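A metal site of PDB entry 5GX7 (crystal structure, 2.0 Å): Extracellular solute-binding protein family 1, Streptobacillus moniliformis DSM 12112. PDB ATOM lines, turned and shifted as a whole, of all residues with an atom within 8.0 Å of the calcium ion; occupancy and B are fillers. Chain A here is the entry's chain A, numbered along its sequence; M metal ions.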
ATOM      1  N   TRP A 146     -18.022 -16.708 -20.229  1.00  0.00           N
ATOM      2  CA  TRP A 146     -17.868 -17.095 -21.632  1.00  0.00           C
ATOM      3  C   TRP A 146     -17.680 -15.868 -22.548  1.00  0.00           C
ATOM      4  O   TRP A 146     -16.836 -15.901 -23.459  1.00  0.00           O
ATOM      5  CB  TRP A 146     -19.087 -17.898 -22.051  1.00  0.00           C
ATOM      6  CG  TRP A 146     -19.081 -19.260 -21.473  1.00  0.00           C
ATOM      7  CD1 TRP A 146     -18.148 -19.814 -20.589  1.00  0.00           C
ATOM      8  CD2 TRP A 146     -19.989 -20.328 -21.832  1.00  0.00           C
ATOM      9  NE1 TRP A 146     -18.441 -21.136 -20.378  1.00  0.00           N
ATOM     10  CE2 TRP A 146     -19.577 -21.470 -21.110  1.00  0.00           C
ATOM     11  CE3 TRP A 146     -21.085 -20.416 -22.694  1.00  0.00           C
ATOM     12  CZ2 TRP A 146     -20.222 -22.658 -21.226  1.00  0.00           C
ATOM     13  CZ3 TRP A 146     -21.769 -21.643 -22.789  1.00  0.00           C
ATOM     14  CH2 TRP A 146     -21.338 -22.743 -22.058  1.00  0.00           C
ATOM     15  N   PHE A 168     -21.007 -18.900 -28.950  1.00  0.00           N
ATOM     16  CA  PHE A 168     -21.048 -19.934 -27.897  1.00  0.00           C
ATOM     17  C   PHE A 168     -21.150 -21.331 -28.492  1.00  0.00           C
ATOM     18  O   PHE A 168     -20.559 -22.282 -27.982  1.00  0.00           O
ATOM     19  CB  PHE A 168     -22.273 -19.757 -26.979  1.00  0.00           C
ATOM     20  CG  PHE A 168     -22.181 -18.613 -26.008  1.00  0.00           C
ATOM     21  CD1 PHE A 168     -21.013 -17.845 -25.913  1.00  0.00           C
ATOM     22  CD2 PHE A 168     -23.271 -18.297 -25.205  1.00  0.00           C
ATOM     23  CE1 PHE A 168     -20.943 -16.781 -24.968  1.00  0.00           C
ATOM     24  CE2 PHE A 168     -23.218 -17.223 -24.246  1.00  0.00           C
ATOM     25  CZ  PHE A 168     -22.071 -16.465 -24.127  1.00  0.00           C
ATOM     26  N   ARG A 169     -21.965 -21.482 -29.539  1.00  0.00           N
ATOM     27  CA  ARG A 169     -22.163 -22.791 -30.141  1.00  0.00           C
ATOM     28  C   ARG A 169     -20.914 -23.228 -30.890  1.00  0.00           C
ATOM     29  O   ARG A 169     -20.539 -24.396 -30.827  1.00  0.00           O
ATOM     30  CB  ARG A 169     -23.354 -22.770 -31.090  1.00  0.00           C
ATOM     31  CG  ARG A 169     -23.652 -24.122 -31.772  1.00  0.00           C
ATOM     32  CD  ARG A 169     -23.944 -25.237 -30.801  1.00  0.00           C
ATOM     33  NE  ARG A 169     -24.119 -26.504 -31.547  1.00  0.00           N
ATOM     34  CZ  ARG A 169     -23.945 -27.714 -31.034  1.00  0.00           C
ATOM     35  NH1 ARG A 169     -23.603 -27.860 -29.721  1.00  0.00           N
ATOM     36  NH2 ARG A 169     -24.170 -28.789 -31.815  1.00  0.00           N
ATOM     37  N   GLU A 170     -20.249 -22.298 -31.581  1.00  0.00           N
ATOM     38  CA  GLU A 170     -19.199 -22.685 -32.512  1.00  0.00           C
ATOM     39  C   GLU A 170     -17.801 -22.624 -31.916  1.00  0.00           C
ATOM     40  O   GLU A 170     -16.905 -23.264 -32.467  1.00  0.00           O
ATOM     41  CB  GLU A 170     -19.243 -21.800 -33.769  1.00  0.00           C
ATOM     42  CG  GLU A 170     -20.597 -21.976 -34.545  1.00  0.00           C
ATOM     43  CD  GLU A 170     -20.752 -23.439 -35.089  1.00  0.00           C
ATOM     44  OE1 GLU A 170     -19.711 -24.090 -35.417  1.00  0.00           O
ATOM     45  OE2 GLU A 170     -21.893 -23.975 -35.118  1.00  0.00           O
ATOM     46  N   LYS A 171     -17.583 -21.902 -30.810  1.00  0.00           N
ATOM     47  CA  LYS A 171     -16.223 -21.599 -30.391  1.00  0.00           C
ATOM     48  C   LYS A 171     -15.826 -22.151 -29.038  1.00  0.00           C
ATOM     49  O   LYS A 171     -14.900 -21.596 -28.404  1.00  0.00           O
ATOM     50  CB  LYS A 171     -15.989 -20.098 -30.408  1.00  0.00           C
ATOM     51  CG  LYS A 171     -16.210 -19.448 -31.760  1.00  0.00           C
ATOM     52  CD  LYS A 171     -15.904 -17.992 -31.555  1.00  0.00           C
ATOM     53  CE  LYS A 171     -16.104 -17.122 -32.810  1.00  0.00           C
ATOM     54  NZ  LYS A 171     -15.769 -17.756 -34.092  1.00  0.00           N
ATOM     55  N   ASP A 172     -16.495 -23.209 -28.559  1.00  0.00           N
ATOM     56  CA  ASP A 172     -16.019 -24.006 -27.427  1.00  0.00           C
ATOM     57  C   ASP A 172     -15.666 -23.144 -26.204  1.00  0.00           C
ATOM     58  O   ASP A 172     -14.578 -23.263 -25.635  1.00  0.00           O
ATOM     59  CB  ASP A 172     -14.809 -24.827 -27.884  1.00  0.00           C
ATOM     60  CG  ASP A 172     -14.384 -25.917 -26.887  1.00  0.00           C
ATOM     61  OD1 ASP A 172     -15.241 -26.573 -26.241  1.00  0.00           O
ATOM     62  OD2 ASP A 172     -13.168 -26.109 -26.748  1.00  0.00           O
ATOM     63  N   PRO A 173     -16.579 -22.270 -25.767  1.00  0.00           N
ATOM     64  CA  PRO A 173     -16.245 -21.405 -24.629  1.00  0.00           C
ATOM     65  C   PRO A 173     -16.024 -22.195 -23.346  1.00  0.00           C
ATOM     66  O   PRO A 173     -15.198 -21.764 -22.548  1.00  0.00           O
ATOM     67  CB  PRO A 173     -17.435 -20.459 -24.547  1.00  0.00           C
ATOM     68  CG  PRO A 173     -18.532 -21.222 -25.116  1.00  0.00           C
ATOM     69  CD  PRO A 173     -17.936 -21.942 -26.263  1.00  0.00           C
ATOM     70  N   ASN A 174     -16.590 -23.390 -23.191  1.00  0.00           N
ATOM     71  CA  ASN A 174     -16.235 -24.128 -21.986  1.00  0.00           C
ATOM     72  C   ASN A 174     -14.871 -24.821 -22.130  1.00  0.00           C
ATOM     73  O   ASN A 174     -14.424 -25.453 -21.183  1.00  0.00           O
ATOM     74  CB  ASN A 174     -17.352 -25.145 -21.603  1.00  0.00           C
ATOM     75  CG  ASN A 174     -17.491 -26.318 -22.589  1.00  0.00           C
ATOM     76  OD1 ASN A 174     -16.608 -26.617 -23.371  1.00  0.00           O
ATOM     77  ND2 ASN A 174     -18.608 -26.993 -22.524  1.00  0.00           N
ATOM     78  N   GLY A 175     -14.179 -24.685 -23.268  1.00  0.00           N
ATOM     79  CA  GLY A 175     -12.760 -25.054 -23.327  1.00  0.00           C
ATOM     80  C   GLY A 175     -12.475 -26.542 -23.372  1.00  0.00           C
ATOM     81  O   GLY A 175     -11.331 -26.941 -23.198  1.00  0.00           O
ATOM     82  N   ASN A 176     -13.449 -27.395 -23.629  1.00  0.00           N
ATOM     83  CA  ASN A 176     -13.177 -28.838 -23.502  1.00  0.00           C
ATOM     84  C   ASN A 176     -12.933 -29.529 -24.850  1.00  0.00           C
ATOM     85  O   ASN A 176     -12.946 -30.779 -24.916  1.00  0.00           O
ATOM     86  CB  ASN A 176     -14.303 -29.560 -22.762  1.00  0.00           C
ATOM     87  CG  ASN A 176     -15.647 -29.463 -23.470  1.00  0.00           C
ATOM     88  OD1 ASN A 176     -15.748 -29.077 -24.623  1.00  0.00           O
ATOM     89  ND2 ASN A 176     -16.682 -29.904 -22.793  1.00  0.00           N
ATOM     90  N   GLY A 177     -12.769 -28.757 -25.927  1.00  0.00           N
ATOM     91  CA  GLY A 177     -12.560 -29.381 -27.230  1.00  0.00           C
ATOM     92  C   GLY A 177     -13.735 -30.164 -27.781  1.00  0.00           C
ATOM     93  O   GLY A 177     -13.560 -30.854 -28.787  1.00  0.00           O
ATOM     94  N   LYS A 178     -14.940 -30.040 -27.187  1.00  0.00           N
ATOM     95  CA  LYS A 178     -16.127 -30.720 -27.706  1.00  0.00           C
ATOM     96  C   LYS A 178     -17.158 -29.676 -28.139  1.00  0.00           C
ATOM     97  O   LYS A 178     -17.274 -28.619 -27.508  1.00  0.00           O
ATOM     98  CB  LYS A 178     -16.804 -31.634 -26.645  1.00  0.00           C
ATOM     99  CG  LYS A 178     -15.944 -32.732 -26.141  1.00  0.00           C
ATOM    100  CD  LYS A 178     -16.723 -33.837 -25.446  1.00  0.00           C
ATOM    101  CE  LYS A 178     -16.181 -34.054 -24.025  1.00  0.00           C
ATOM    102  NZ  LYS A 178     -14.665 -34.342 -23.903  1.00  0.00           N
ATOM    103  N   LYS A 179     -17.925 -29.999 -29.193  1.00  0.00           N
ATOM    104  CA  LYS A 179     -18.990 -29.086 -29.626  1.00  0.00           C
ATOM    105  C   LYS A 179     -20.239 -29.438 -28.826  1.00  0.00           C
ATOM    106  O   LYS A 179     -21.217 -30.008 -29.339  1.00  0.00           O
ATOM    107  CB  LYS A 179     -19.221 -29.196 -31.122  1.00  0.00           C
ATOM    108  CG  LYS A 179     -20.147 -28.113 -31.719  1.00  0.00           C
ATOM    109  CD  LYS A 179     -20.363 -28.378 -33.238  1.00  0.00           C
ATOM    110  CE  LYS A 179     -21.190 -27.286 -33.950  1.00  0.00           C
ATOM    111  NZ  LYS A 179     -21.513 -27.656 -35.380  1.00  0.00           N
ATOM    112  N   ASP A 180     -20.177 -29.101 -27.528  1.00  0.00           N
ATOM    113  CA  ASP A 180     -21.239 -29.528 -26.625  1.00  0.00           C
ATOM    114  C   ASP A 180     -22.104 -28.383 -26.088  1.00  0.00           C
ATOM    115  O   ASP A 180     -23.093 -28.640 -25.391  1.00  0.00           O
ATOM    116  CB  ASP A 180     -20.658 -30.364 -25.474  1.00  0.00           C
ATOM    117  CG  ASP A 180     -19.657 -29.650 -24.635  1.00  0.00           C
ATOM    118  OD1 ASP A 180     -19.157 -28.529 -24.976  1.00  0.00           O
ATOM    119  OD2 ASP A 180     -19.371 -30.303 -23.588  1.00  0.00           O
ATOM    120  N   GLU A 181     -21.789 -27.150 -26.445  1.00  0.00           N
ATOM    121  CA  GLU A 181     -22.497 -26.026 -25.849  1.00  0.00           C
ATOM    122  C   GLU A 181     -23.982 -25.965 -26.192  1.00  0.00           C
ATOM    123  O   GLU A 181     -24.400 -26.222 -27.316  1.00  0.00           O
ATOM    124  CB  GLU A 181     -21.799 -24.731 -26.253  1.00  0.00           C
ATOM    125  CG  GLU A 181     -20.559 -24.440 -25.327  1.00  0.00           C
ATOM    126  CD  GLU A 181     -19.258 -25.160 -25.724  1.00  0.00           C
ATOM    127  OE1 GLU A 181     -19.234 -25.923 -26.741  1.00  0.00           O
ATOM    128  OE2 GLU A 181     -18.226 -24.975 -24.980  1.00  0.00           O
ATOM    129  N   VAL A 182     -24.761 -25.594 -25.194  1.00  0.00           N
ATOM    130  CA  VAL A 182     -26.182 -25.328 -25.382  1.00  0.00           C
ATOM    131  C   VAL A 182     -26.379 -23.837 -25.155  1.00  0.00           C
ATOM    132  O   VAL A 182     -26.549 -23.417 -24.003  1.00  0.00           O
ATOM    133  CB  VAL A 182     -26.990 -26.200 -24.412  1.00  0.00           C
ATOM    134  CG1 VAL A 182     -28.491 -25.888 -24.539  1.00  0.00           C
ATOM    135  CG2 VAL A 182     -26.705 -27.676 -24.752  1.00  0.00           C
ATOM    136  N   ASN A 259     -21.660 -27.296 -17.117  1.00  0.00           N
ATOM    137  CA  ASN A 259     -20.986 -26.263 -17.913  1.00  0.00           C
ATOM    138  C   ASN A 259     -21.338 -26.313 -19.406  1.00  0.00           C
ATOM    139  O   ASN A 259     -20.466 -26.105 -20.266  1.00  0.00           O
ATOM    140  CB  ASN A 259     -19.469 -26.308 -17.776  1.00  0.00           C
ATOM    141  CG  ASN A 259     -18.822 -24.931 -17.914  1.00  0.00           C
ATOM    142  OD1 ASN A 259     -19.520 -23.883 -17.895  1.00  0.00           O
ATOM    143  ND2 ASN A 259     -17.456 -24.904 -18.081  1.00  0.00           N
ATOM    144  N   LEU A 260     -22.610 -26.564 -19.743  1.00  0.00           N
ATOM    145  CA  LEU A 260     -23.082 -26.558 -21.139  1.00  0.00           C
ATOM    146  C   LEU A 260     -23.910 -25.336 -21.511  1.00  0.00           C
ATOM    147  O   LEU A 260     -23.932 -24.965 -22.691  1.00  0.00           O
ATOM    148  CB  LEU A 260     -23.945 -27.803 -21.443  1.00  0.00           C
ATOM    149  CG  LEU A 260     -23.307 -29.153 -21.089  1.00  0.00           C
ATOM    150  CD1 LEU A 260     -24.397 -30.325 -21.234  1.00  0.00           C
ATOM    151  CD2 LEU A 260     -22.052 -29.503 -21.958  1.00  0.00           C
HETATM  152 CA    CA M   1     -17.253 -27.335 -25.554  1.00  0.00          CA
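Of the 18 residues printed, 6 come within 4 Å of the calcium ion. The nearest printed residue that does not touch the calcium ion is Lys 179 (4.6 Å).
The calcium ion is bound by OD1 of Asp 172, at 2.3 Å. OD1 of Asp 180 binds the calcium ion. O of Lys 178 binds the calcium ion (2.3 Å). The calcium ion is bound by OD1 of Asn 174 (2.4 Å). OD1 of Asn 176 binds the calcium ion. OE2 of Glu 181 binds the calcium ion (2.6 Å). The calcium ion is bound by OE1 of Glu 181.
OD2 of Asp 172 sits at hydrogen-bond distance from N of Gly 177 (2.8 Å). O of Asn 259 sits at hydrogen-bond distance from ND2 of Asn 174 (3.1 Å). The guanidinium group of Arg 169 is in hydrogen-bond range of the backbone carbonyl oxygen of Glu 181, at 3.0 Å.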
